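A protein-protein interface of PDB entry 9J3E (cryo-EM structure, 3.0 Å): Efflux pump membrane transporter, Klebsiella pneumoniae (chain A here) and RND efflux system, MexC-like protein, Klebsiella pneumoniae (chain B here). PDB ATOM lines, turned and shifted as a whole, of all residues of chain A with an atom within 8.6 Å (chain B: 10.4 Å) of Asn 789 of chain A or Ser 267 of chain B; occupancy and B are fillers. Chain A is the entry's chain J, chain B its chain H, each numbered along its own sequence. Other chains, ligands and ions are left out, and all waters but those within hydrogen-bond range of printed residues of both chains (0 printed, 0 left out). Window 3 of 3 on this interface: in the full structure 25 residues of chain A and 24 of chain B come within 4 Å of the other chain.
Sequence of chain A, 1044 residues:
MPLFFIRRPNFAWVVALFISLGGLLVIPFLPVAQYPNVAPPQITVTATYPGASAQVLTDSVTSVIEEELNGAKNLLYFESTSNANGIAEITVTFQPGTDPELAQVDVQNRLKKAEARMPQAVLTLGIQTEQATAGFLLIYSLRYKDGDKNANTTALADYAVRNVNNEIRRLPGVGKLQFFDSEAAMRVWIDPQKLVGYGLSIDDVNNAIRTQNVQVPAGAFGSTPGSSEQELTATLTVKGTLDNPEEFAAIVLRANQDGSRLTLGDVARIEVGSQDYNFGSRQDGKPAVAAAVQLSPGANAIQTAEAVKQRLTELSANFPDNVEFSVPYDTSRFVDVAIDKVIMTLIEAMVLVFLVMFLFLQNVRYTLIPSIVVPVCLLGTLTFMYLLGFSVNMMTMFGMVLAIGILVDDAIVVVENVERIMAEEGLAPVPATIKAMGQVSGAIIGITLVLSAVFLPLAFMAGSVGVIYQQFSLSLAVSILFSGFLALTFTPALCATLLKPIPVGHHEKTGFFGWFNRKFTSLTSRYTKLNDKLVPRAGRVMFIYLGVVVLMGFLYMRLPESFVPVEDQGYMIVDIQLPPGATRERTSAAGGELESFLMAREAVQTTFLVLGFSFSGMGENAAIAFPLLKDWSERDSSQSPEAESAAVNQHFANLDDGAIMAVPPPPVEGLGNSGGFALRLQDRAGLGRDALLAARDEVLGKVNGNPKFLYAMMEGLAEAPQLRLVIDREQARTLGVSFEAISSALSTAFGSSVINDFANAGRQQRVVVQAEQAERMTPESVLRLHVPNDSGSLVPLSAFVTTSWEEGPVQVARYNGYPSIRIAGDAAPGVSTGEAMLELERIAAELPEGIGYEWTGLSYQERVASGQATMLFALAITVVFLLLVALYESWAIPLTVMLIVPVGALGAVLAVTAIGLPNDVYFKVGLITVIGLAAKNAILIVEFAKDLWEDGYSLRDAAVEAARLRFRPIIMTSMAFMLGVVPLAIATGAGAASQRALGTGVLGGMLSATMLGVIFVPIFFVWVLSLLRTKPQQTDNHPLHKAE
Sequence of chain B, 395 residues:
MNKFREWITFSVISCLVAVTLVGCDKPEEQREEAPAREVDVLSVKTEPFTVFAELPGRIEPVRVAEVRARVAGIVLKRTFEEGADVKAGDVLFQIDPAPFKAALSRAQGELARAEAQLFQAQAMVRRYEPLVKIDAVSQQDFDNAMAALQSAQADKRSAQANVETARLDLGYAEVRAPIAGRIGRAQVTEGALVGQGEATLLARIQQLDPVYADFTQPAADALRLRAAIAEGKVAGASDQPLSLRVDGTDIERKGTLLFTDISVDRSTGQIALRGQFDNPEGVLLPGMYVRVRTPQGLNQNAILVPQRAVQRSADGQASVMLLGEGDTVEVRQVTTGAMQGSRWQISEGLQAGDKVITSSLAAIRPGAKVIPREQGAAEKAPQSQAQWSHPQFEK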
ATOM      1  N   SER A 201     -26.960   4.114  -7.655  1.00  0.00           N
ATOM      2  CA  SER A 201     -26.249   5.004  -6.757  1.00  0.00           C
ATOM      3  C   SER A 201     -27.065   6.262  -6.506  1.00  0.00           C
ATOM      4  O   SER A 201     -28.043   6.548  -7.198  1.00  0.00           O
ATOM      5  CB  SER A 201     -24.889   5.372  -7.334  1.00  0.00           C
ATOM      6  OG  SER A 201     -25.035   6.164  -8.495  1.00  0.00           O
ATOM      7  N   GLN A 731      -6.783   3.681  -2.930  1.00  0.00           N
ATOM      8  CA  GLN A 731      -7.547   2.437  -2.939  1.00  0.00           C
ATOM      9  C   GLN A 731      -8.893   2.620  -3.612  1.00  0.00           C
ATOM     10  O   GLN A 731      -9.279   1.820  -4.471  1.00  0.00           O
ATOM     11  CB  GLN A 731      -7.756   1.931  -1.519  1.00  0.00           C
ATOM     12  CG  GLN A 731      -8.016   0.453  -1.436  1.00  0.00           C
ATOM     13  CD  GLN A 731      -8.070  -0.031  -0.016  1.00  0.00           C
ATOM     14  OE1 GLN A 731      -7.612   0.648   0.897  1.00  0.00           O
ATOM     15  NE2 GLN A 731      -8.645  -1.207   0.187  1.00  0.00           N
ATOM     16  N   ALA A 732      -9.620   3.669  -3.242  1.00  0.00           N
ATOM     17  CA  ALA A 732     -10.922   3.895  -3.842  1.00  0.00           C
ATOM     18  C   ALA A 732     -10.793   4.091  -5.340  1.00  0.00           C
ATOM     19  O   ALA A 732     -11.593   3.558  -6.115  1.00  0.00           O
ATOM     20  CB  ALA A 732     -11.594   5.104  -3.196  1.00  0.00           C
ATOM     21  N   ARG A 733      -9.776   4.833  -5.767  1.00  0.00           N
ATOM     22  CA  ARG A 733      -9.594   5.090  -7.188  1.00  0.00           C
ATOM     23  C   ARG A 733      -9.287   3.811  -7.952  1.00  0.00           C
ATOM     24  O   ARG A 733      -9.824   3.591  -9.043  1.00  0.00           O
ATOM     25  CB  ARG A 733      -8.481   6.107  -7.381  1.00  0.00           C
ATOM     26  CG  ARG A 733      -8.380   6.655  -8.772  1.00  0.00           C
ATOM     27  CD  ARG A 733      -9.597   7.447  -9.156  1.00  0.00           C
ATOM     28  NE  ARG A 733      -9.323   8.229 -10.351  1.00  0.00           N
ATOM     29  CZ  ARG A 733     -10.251   8.776 -11.120  1.00  0.00           C
ATOM     30  NH1 ARG A 733     -11.539   8.625 -10.862  1.00  0.00           N
ATOM     31  NH2 ARG A 733      -9.878   9.493 -12.175  1.00  0.00           N
ATOM     32  N   THR A 734      -8.433   2.953  -7.394  1.00  0.00           N
ATOM     33  CA  THR A 734      -8.074   1.717  -8.079  1.00  0.00           C
ATOM     34  C   THR A 734      -9.285   0.821  -8.271  1.00  0.00           C
ATOM     35  O   THR A 734      -9.453   0.211  -9.332  1.00  0.00           O
ATOM     36  CB  THR A 734      -6.979   0.992  -7.306  1.00  0.00           C
ATOM     37  OG1 THR A 734      -5.777   1.768  -7.358  1.00  0.00           O
ATOM     38  CG2 THR A 734      -6.728  -0.378  -7.886  1.00  0.00           C
ATOM     39  N   LEU A 735     -10.144   0.749  -7.285  1.00  0.00           N
ATOM     40  CA  LEU A 735     -11.393   0.040  -7.496  1.00  0.00           C
ATOM     41  C   LEU A 735     -12.283   0.729  -8.511  1.00  0.00           C
ATOM     42  O   LEU A 735     -13.359   0.219  -8.818  1.00  0.00           O
ATOM     43  CB  LEU A 735     -12.136  -0.107  -6.169  1.00  0.00           C
ATOM     44  CG  LEU A 735     -11.381  -0.815  -5.048  1.00  0.00           C
ATOM     45  CD1 LEU A 735     -12.121  -0.653  -3.747  1.00  0.00           C
ATOM     46  CD2 LEU A 735     -11.188  -2.272  -5.359  1.00  0.00           C
ATOM     47  N   GLY A 736     -11.868   1.869  -9.054  1.00  0.00           N
ATOM     48  CA  GLY A 736     -12.673   2.582 -10.019  1.00  0.00           C
ATOM     49  C   GLY A 736     -13.636   3.578  -9.429  1.00  0.00           C
ATOM     50  O   GLY A 736     -14.576   3.992 -10.113  1.00  0.00           O
ATOM     51  N   VAL A 737     -13.429   3.992  -8.186  1.00  0.00           N
ATOM     52  CA  VAL A 737     -14.350   4.881  -7.492  1.00  0.00           C
ATOM     53  C   VAL A 737     -13.793   6.291  -7.546  1.00  0.00           C
ATOM     54  O   VAL A 737     -12.704   6.556  -7.027  1.00  0.00           O
ATOM     55  CB  VAL A 737     -14.557   4.444  -6.039  1.00  0.00           C
ATOM     56  CG1 VAL A 737     -15.611   5.304  -5.394  1.00  0.00           C
ATOM     57  CG2 VAL A 737     -14.911   2.982  -5.978  1.00  0.00           C
ATOM     58  N   SER A 738     -14.538   7.202  -8.154  1.00  0.00           N
ATOM     59  CA  SER A 738     -14.141   8.597  -8.162  1.00  0.00           C
ATOM     60  C   SER A 738     -14.373   9.209  -6.791  1.00  0.00           C
ATOM     61  O   SER A 738     -15.258   8.787  -6.044  1.00  0.00           O
ATOM     62  CB  SER A 738     -14.931   9.377  -9.207  1.00  0.00           C
ATOM     63  OG  SER A 738     -16.190   9.767  -8.689  1.00  0.00           O
ATOM     64  N   ALA A 741     -17.910  10.616  -6.646  1.00  0.00           N
ATOM     65  CA  ALA A 741     -18.987   9.721  -6.238  1.00  0.00           C
ATOM     66  C   ALA A 741     -19.075   9.614  -4.724  1.00  0.00           C
ATOM     67  O   ALA A 741     -20.167   9.691  -4.155  1.00  0.00           O
ATOM     68  CB  ALA A 741     -18.790   8.343  -6.861  1.00  0.00           C
ATOM     69  N   HIS A 786     -22.911   2.433  -0.350  1.00  0.00           N
ATOM     70  CA  HIS A 786     -22.197   1.974  -1.529  1.00  0.00           C
ATOM     71  C   HIS A 786     -22.093   3.098  -2.544  1.00  0.00           C
ATOM     72  O   HIS A 786     -22.958   3.973  -2.617  1.00  0.00           O
ATOM     73  CB  HIS A 786     -22.878   0.780  -2.180  1.00  0.00           C
ATOM     74  CG  HIS A 786     -22.800  -0.473  -1.371  1.00  0.00           C
ATOM     75  ND1 HIS A 786     -23.256  -0.551  -0.075  1.00  0.00           N
ATOM     76  CD2 HIS A 786     -22.347  -1.708  -1.687  1.00  0.00           C
ATOM     77  CE1 HIS A 786     -23.072  -1.777   0.380  1.00  0.00           C
ATOM     78  NE2 HIS A 786     -22.522  -2.498  -0.579  1.00  0.00           N
ATOM     79  N   VAL A 787     -21.027   3.057  -3.331  1.00  0.00           N
ATOM     80  CA  VAL A 787     -20.803   4.035  -4.389  1.00  0.00           C
ATOM     81  C   VAL A 787     -20.484   3.269  -5.664  1.00  0.00           C
ATOM     82  O   VAL A 787     -19.988   2.137  -5.590  1.00  0.00           O
ATOM     83  CB  VAL A 787     -19.672   4.997  -4.020  1.00  0.00           C
ATOM     84  CG1 VAL A 787     -20.141   5.953  -2.960  1.00  0.00           C
ATOM     85  CG2 VAL A 787     -18.493   4.218  -3.524  1.00  0.00           C
ATOM     86  N   PRO A 788     -20.753   3.820  -6.839  1.00  0.00           N
ATOM     87  CA  PRO A 788     -20.484   3.087  -8.073  1.00  0.00           C
ATOM     88  C   PRO A 788     -19.077   3.328  -8.584  1.00  0.00           C
ATOM     89  O   PRO A 788     -18.527   4.427  -8.489  1.00  0.00           O
ATOM     90  CB  PRO A 788     -21.518   3.660  -9.044  1.00  0.00           C
ATOM     91  CG  PRO A 788     -21.650   5.061  -8.607  1.00  0.00           C
ATOM     92  CD  PRO A 788     -21.463   5.079  -7.106  1.00  0.00           C
ATOM     93  N   ASN A 789     -18.504   2.279  -9.157  1.00  0.00           N
ATOM     94  CA  ASN A 789     -17.206   2.360  -9.797  1.00  0.00           C
ATOM     95  C   ASN A 789     -17.397   2.611 -11.286  1.00  0.00           C
ATOM     96  O   ASN A 789     -18.510   2.830 -11.766  1.00  0.00           O
ATOM     97  CB  ASN A 789     -16.404   1.090  -9.530  1.00  0.00           C
ATOM     98  CG  ASN A 789     -17.103  -0.149 -10.018  1.00  0.00           C
ATOM     99  OD1 ASN A 789     -18.201  -0.083 -10.562  1.00  0.00           O
ATOM    100  ND2 ASN A 789     -16.476  -1.296  -9.815  1.00  0.00           N
ATOM    101  N   ASP A 790     -16.295   2.586 -12.033  1.00  0.00           N
ATOM    102  CA  ASP A 790     -16.405   2.857 -13.461  1.00  0.00           C
ATOM    103  C   ASP A 790     -17.043   1.696 -14.215  1.00  0.00           C
ATOM    104  O   ASP A 790     -17.644   1.904 -15.274  1.00  0.00           O
ATOM    105  CB  ASP A 790     -15.034   3.240 -14.034  1.00  0.00           C
ATOM    106  CG  ASP A 790     -14.096   2.053 -14.252  1.00  0.00           C
ATOM    107  OD1 ASP A 790     -14.526   0.887 -14.361  1.00  0.00           O
ATOM    108  OD2 ASP A 790     -12.876   2.306 -14.329  1.00  0.00           O
ATOM    109  N   SER A 791     -16.937   0.480 -13.689  1.00  0.00           N
ATOM    110  CA  SER A 791     -17.430  -0.706 -14.374  1.00  0.00           C
ATOM    111  C   SER A 791     -18.898  -0.994 -14.096  1.00  0.00           C
ATOM    112  O   SER A 791     -19.421  -1.992 -14.597  1.00  0.00           O
ATOM    113  CB  SER A 791     -16.590  -1.922 -13.986  1.00  0.00           C
ATOM    114  OG  SER A 791     -16.913  -2.358 -12.680  1.00  0.00           O
ATOM    115  N   GLY A 792     -19.571  -0.155 -13.317  1.00  0.00           N
ATOM    116  CA  GLY A 792     -20.993  -0.296 -13.092  1.00  0.00           C
ATOM    117  C   GLY A 792     -21.400  -1.038 -11.837  1.00  0.00           C
ATOM    118  O   GLY A 792     -22.582  -1.003 -11.478  1.00  0.00           O
ATOM    119  N   SER A 793     -20.475  -1.703 -11.160  1.00  0.00           N
ATOM    120  CA  SER A 793     -20.799  -2.336  -9.894  1.00  0.00           C
ATOM    121  C   SER A 793     -20.840  -1.293  -8.787  1.00  0.00           C
ATOM    122  O   SER A 793     -20.393  -0.158  -8.956  1.00  0.00           O
ATOM    123  CB  SER A 793     -19.781  -3.421  -9.556  1.00  0.00           C
ATOM    124  OG  SER A 793     -19.783  -4.440 -10.535  1.00  0.00           O
ATOM    125  N   LEU A 794     -21.393  -1.682  -7.645  1.00  0.00           N
ATOM    126  CA  LEU A 794     -21.459  -0.808  -6.484  1.00  0.00           C
ATOM    127  C   LEU A 794     -20.421  -1.234  -5.461  1.00  0.00           C
ATOM    128  O   LEU A 794     -20.365  -2.404  -5.076  1.00  0.00           O
ATOM    129  CB  LEU A 794     -22.849  -0.821  -5.858  1.00  0.00           C
ATOM    130  CG  LEU A 794     -23.910  -0.195  -6.748  1.00  0.00           C
ATOM    131  CD1 LEU A 794     -25.251  -0.220  -6.062  1.00  0.00           C
ATOM    132  CD2 LEU A 794     -23.508   1.213  -7.089  1.00  0.00           C
ATOM    133  N   VAL A 795     -19.610  -0.284  -5.026  1.00  0.00           N
ATOM    134  CA  VAL A 795     -18.536  -0.519  -4.066  1.00  0.00           C
ATOM    135  C   VAL A 795     -19.013  -0.056  -2.698  1.00  0.00           C
ATOM    136  O   VAL A 795     -19.387   1.113  -2.553  1.00  0.00           O
ATOM    137  CB  VAL A 795     -17.247   0.219  -4.462  1.00  0.00           C
ATOM    138  CG1 VAL A 795     -16.122  -0.186  -3.550  1.00  0.00           C
ATOM    139  CG2 VAL A 795     -16.898  -0.075  -5.904  1.00  0.00           C
ATOM    140  N   PRO A 796     -19.030  -0.919  -1.689  1.00  0.00           N
ATOM    141  CA  PRO A 796     -19.376  -0.460  -0.344  1.00  0.00           C
ATOM    142  C   PRO A 796     -18.333   0.514   0.154  1.00  0.00           C
ATOM    143  O   PRO A 796     -17.161   0.435  -0.214  1.00  0.00           O
ATOM    144  CB  PRO A 796     -19.367  -1.744   0.484  1.00  0.00           C
ATOM    145  CG  PRO A 796     -18.437  -2.630  -0.239  1.00  0.00           C
ATOM    146  CD  PRO A 796     -18.612  -2.326  -1.694  1.00  0.00           C
ATOM    147  N   ALA A 799     -15.132  -0.708   2.040  1.00  0.00           N
ATOM    148  CA  ALA A 799     -14.017  -1.271   1.294  1.00  0.00           C
ATOM    149  C   ALA A 799     -12.825  -0.327   1.252  1.00  0.00           C
ATOM    150  O   ALA A 799     -11.698  -0.777   1.037  1.00  0.00           O
ATOM    151  CB  ALA A 799     -14.455  -1.622  -0.124  1.00  0.00           C
ATOM    152  N   PHE A 800     -13.040   0.974   1.432  1.00  0.00           N
ATOM    153  CA  PHE A 800     -11.918   1.895   1.322  1.00  0.00           C
ATOM    154  C   PHE A 800     -11.928   3.032   2.336  1.00  0.00           C
ATOM    155  O   PHE A 800     -11.068   3.913   2.247  1.00  0.00           O
ATOM    156  CB  PHE A 800     -11.849   2.483  -0.085  1.00  0.00           C
ATOM    157  CG  PHE A 800     -13.152   3.025  -0.582  1.00  0.00           C
ATOM    158  CD1 PHE A 800     -13.554   4.300  -0.249  1.00  0.00           C
ATOM    159  CD2 PHE A 800     -13.962   2.272  -1.403  1.00  0.00           C
ATOM    160  CE1 PHE A 800     -14.742   4.801  -0.711  1.00  0.00           C
ATOM    161  CE2 PHE A 800     -15.147   2.774  -1.867  1.00  0.00           C
ATOM    162  CZ  PHE A 800     -15.538   4.037  -1.521  1.00  0.00           C
ATOM    163  N   THR B 216     -22.872 -10.998  -0.492  1.00  0.00           N
ATOM    164  CA  THR B 216     -21.496 -10.547  -0.595  1.00  0.00           C
ATOM    165  C   THR B 216     -21.142  -9.690   0.610  1.00  0.00           C
ATOM    166  O   THR B 216     -21.980  -8.962   1.141  1.00  0.00           O
ATOM    167  CB  THR B 216     -21.289  -9.768  -1.888  1.00  0.00           C
ATOM    168  OG1 THR B 216     -22.086 -10.360  -2.918  1.00  0.00           O
ATOM    169  CG2 THR B 216     -19.854  -9.846  -2.319  1.00  0.00           C
ATOM    170  N   PRO B 218     -17.876  -7.148   2.331  1.00  0.00           N
ATOM    171  CA  PRO B 218     -16.601  -6.469   2.096  1.00  0.00           C
ATOM    172  C   PRO B 218     -15.449  -7.280   2.661  1.00  0.00           C
ATOM    173  O   PRO B 218     -15.585  -7.952   3.683  1.00  0.00           O
ATOM    174  CB  PRO B 218     -16.767  -5.140   2.834  1.00  0.00           C
ATOM    175  CG  PRO B 218     -18.226  -4.923   2.873  1.00  0.00           C
ATOM    176  CD  PRO B 218     -18.843  -6.275   3.011  1.00  0.00           C
ATOM    177  N   ALA B 219     -14.312  -7.226   1.971  1.00  0.00           N
ATOM    178  CA  ALA B 219     -13.166  -8.025   2.386  1.00  0.00           C
ATOM    179  C   ALA B 219     -12.656  -7.601   3.755  1.00  0.00           C
ATOM    180  O   ALA B 219     -12.291  -8.451   4.576  1.00  0.00           O
ATOM    181  CB  ALA B 219     -12.052  -7.919   1.350  1.00  0.00           C
ATOM    182  N   SER B 263     -11.519 -15.578  -2.835  1.00  0.00           N
ATOM    183  CA  SER B 263     -11.045 -14.539  -3.734  1.00  0.00           C
ATOM    184  C   SER B 263     -11.890 -13.282  -3.601  1.00  0.00           C
ATOM    185  O   SER B 263     -13.108 -13.308  -3.789  1.00  0.00           O
ATOM    186  CB  SER B 263     -11.072 -15.026  -5.179  1.00  0.00           C
ATOM    187  OG  SER B 263     -12.404 -15.153  -5.640  1.00  0.00           O
ATOM    188  N   VAL B 264     -11.224 -12.172  -3.317  1.00  0.00           N
ATOM    189  CA  VAL B 264     -11.866 -10.875  -3.181  1.00  0.00           C
ATOM    190  C   VAL B 264     -12.114 -10.325  -4.572  1.00  0.00           C
ATOM    191  O   VAL B 264     -11.209 -10.323  -5.414  1.00  0.00           O
ATOM    192  CB  VAL B 264     -10.994  -9.913  -2.364  1.00  0.00           C
ATOM    193  CG1 VAL B 264     -11.627  -8.547  -2.323  1.00  0.00           C
ATOM    194  CG2 VAL B 264     -10.791 -10.451  -0.968  1.00  0.00           C
ATOM    195  N   ASP B 265     -13.338  -9.875  -4.821  1.00  0.00           N
ATOM    196  CA  ASP B 265     -13.651  -9.251  -6.097  1.00  0.00           C
ATOM    197  C   ASP B 265     -12.740  -8.054  -6.319  1.00  0.00           C
ATOM    198  O   ASP B 265     -12.578  -7.214  -5.431  1.00  0.00           O
ATOM    199  CB  ASP B 265     -15.114  -8.824  -6.124  1.00  0.00           C
ATOM    200  CG  ASP B 265     -15.537  -8.289  -7.471  1.00  0.00           C
ATOM    201  OD1 ASP B 265     -15.187  -7.136  -7.791  1.00  0.00           O
ATOM    202  OD2 ASP B 265     -16.233  -9.015  -8.208  1.00  0.00           O
ATOM    203  N   ARG B 266     -12.130  -7.985  -7.500  1.00  0.00           N
ATOM    204  CA  ARG B 266     -11.211  -6.891  -7.782  1.00  0.00           C
ATOM    205  C   ARG B 266     -11.930  -5.561  -7.936  1.00  0.00           C
ATOM    206  O   ARG B 266     -11.395  -4.524  -7.535  1.00  0.00           O
ATOM    207  CB  ARG B 266     -10.403  -7.196  -9.037  1.00  0.00           C
ATOM    208  CG  ARG B 266      -9.001  -6.653  -8.997  1.00  0.00           C
ATOM    209  CD  ARG B 266      -8.150  -7.254 -10.091  1.00  0.00           C
ATOM    210  NE  ARG B 266      -7.888  -8.665  -9.845  1.00  0.00           N
ATOM    211  CZ  ARG B 266      -6.681  -9.169  -9.638  1.00  0.00           C
ATOM    212  NH1 ARG B 266      -5.598  -8.413  -9.699  1.00  0.00           N
ATOM    213  NH2 ARG B 266      -6.556 -10.464  -9.372  1.00  0.00           N
ATOM    214  N   SER B 267     -13.122  -5.560  -8.525  1.00  0.00           N
ATOM    215  CA  SER B 267     -13.804  -4.298  -8.778  1.00  0.00           C
ATOM    216  C   SER B 267     -14.434  -3.729  -7.516  1.00  0.00           C
ATOM    217  O   SER B 267     -14.401  -2.515  -7.300  1.00  0.00           O
ATOM    218  CB  SER B 267     -14.863  -4.483  -9.860  1.00  0.00           C
ATOM    219  OG  SER B 267     -15.959  -5.231  -9.370  1.00  0.00           O
ATOM    220  N   THR B 268     -15.009  -4.581  -6.669  1.00  0.00           N
ATOM    221  CA  THR B 268     -15.755  -4.120  -5.509  1.00  0.00           C
ATOM    222  C   THR B 268     -15.070  -4.407  -4.184  1.00  0.00           C
ATOM    223  O   THR B 268     -15.571  -3.967  -3.147  1.00  0.00           O
ATOM    224  CB  THR B 268     -17.149  -4.754  -5.480  1.00  0.00           C
ATOM    225  OG1 THR B 268     -17.021  -6.170  -5.326  1.00  0.00           O
ATOM    226  CG2 THR B 268     -17.882  -4.467  -6.760  1.00  0.00           C
ATOM    227  N   GLY B 269     -13.964  -5.139  -4.182  1.00  0.00           N
ATOM    228  CA  GLY B 269     -13.280  -5.416  -2.936  1.00  0.00           C
ATOM    229  C   GLY B 269     -14.111  -6.188  -1.942  1.00  0.00           C
ATOM    230  O   GLY B 269     -14.058  -5.899  -0.744  1.00  0.00           O
ATOM    231  N   GLN B 270     -14.881  -7.165  -2.405  1.00  0.00           N
ATOM    232  CA  GLN B 270     -15.712  -7.978  -1.535  1.00  0.00           C
ATOM    233  C   GLN B 270     -15.463  -9.455  -1.790  1.00  0.00           C
ATOM    234  O   GLN B 270     -14.969  -9.844  -2.852  1.00  0.00           O
ATOM    235  CB  GLN B 270     -17.197  -7.694  -1.736  1.00  0.00           C
ATOM    236  CG  GLN B 270     -17.548  -6.274  -2.076  1.00  0.00           C
ATOM    237  CD  GLN B 270     -19.041  -6.089  -2.212  1.00  0.00           C
ATOM    238  OE1 GLN B 270     -19.687  -5.494  -1.350  1.00  0.00           O
ATOM    239  NE2 GLN B 270     -19.603  -6.609  -3.292  1.00  0.00           N
ATOM    240  N   ILE B 271     -15.810 -10.270  -0.804  1.00  0.00           N
ATOM    241  CA  ILE B 271     -15.790 -11.721  -0.932  1.00  0.00           C
ATOM    242  C   ILE B 271     -17.223 -12.205  -1.059  1.00  0.00           C
ATOM    243  O   ILE B 271     -18.140 -11.630  -0.463  1.00  0.00           O
ATOM    244  CB  ILE B 271     -15.090 -12.384   0.266  1.00  0.00           C
ATOM    245  CG1 ILE B 271     -15.929 -12.233   1.529  1.00  0.00           C
ATOM    246  CG2 ILE B 271     -13.741 -11.767   0.489  1.00  0.00           C
ATOM    247  CD1 ILE B 271     -15.544 -13.184   2.623  1.00  0.00           C
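The backbone carbonyl oxygen of Ser 267 of chain B lies within hydrogen-bond range of the side-chain amide nitrogen of Asn 789 of chain A (3.5 Å). The backbone carbonyl oxygen (O) of Leu 735 of chain A sits close to the backbone carbonyl oxygen (O) of Ser 267 of chain B.
The side-chain carboxylate (OD1) of Asp 265 of chain B is in hydrogen-bond range of the backbone NH (N) of Thr 268 of chain B (2.8 Å). The backbone NH (N) of Asp 265 of chain B sits at hydrogen-bond distance from the backbone carbonyl oxygen (O) of Gln 270 of chain B, 2.6 Å away. NE2 of Gln 270 of chain B sits close to OG1 of Thr 268 of chain B (3.3 Å). O of Val 787 of chain A is in hydrogen-bond range of N of Val 795 of chain A, at 2.5 Å. OD1 of Asn 789 of chain A is in hydrogen-bond range of N of Gly 792 of chain A, 3.1 Å away. The side-chain amide oxygen (OD1) of Asn 789 of chain A lies close to the backbone carbonyl oxygen (O) of Ser 793 of chain A, 2.7 Å away.
Among the printed residues, pairs that only touch across the chains: Leu 735 of chain A with Arg 266 of chain B, Ser 793 of chain A with Thr 268 of chain B, Leu 794 of chain A with Thr 268 of chain B, Val 795 of chain A with Ser 267 of chain B, Val 795 of chain A with Thr 268 of chain B, Pro 796 of chain A with Pro 218 of chain B, Pro 796 of chain A with Thr 268 of chain B, Pro 796 of chain A with Gln 270 of chain B and Ala 799 of chain A with Thr 268 of chain B.
Thr 734 of chain A touches none of the printed residues of chain B. Leu 735 of chain A touches just these residues of chain B: Arg 266 and Ser 267. No residue of chain B comes within 4 Å of Pro 788 of chain A. No residue of chain B comes within 4 Å of Asp 790 of chain A. No residue of chain B comes within 4 Å of Gly 792 of chain A. Ser 793 of chain A touches just one residue of chain B: Thr 268 (3.5 Å). Printed residues of chain B within 4 Å of Leu 794 of chain A: Thr 268 (3.6 Å). Of the printed residues of chain B, Val 795 of chain A touches Ser 267 and Thr 268. Printed residues of chain B within 4 Å of Pro 796 of chain A: Pro 218, Thr 268 and Gln 270. Printed residues of chain A within 4 Å of Arg 266 of chain B: Leu 735 (3.1 Å). Ser 267 of chain B touches just these residues of chain A: Leu 735 (3.3 Å), Asn 789 (3.5 Å) and Val 795 (3.8 Å). Gly 269 of chain B touches none of the printed residues of chain A. Printed residues of chain A within 4 Å of Gln 270 of chain B: Pro 796 (3.3 Å).
Hydrophobic or aromatic side chains of chain A within 4 Å of the printed part of chain B: Leu 735, Val 795, Pro 796 and Ala 799. Of the 12 printed residues of chain B, 5 touch a printed residue of chain A. Hydrophobic or aromatic side chains of chain B that line the printed part of chain A: Pro 218. Among the printed residues, 11 pairs touch across the chains.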
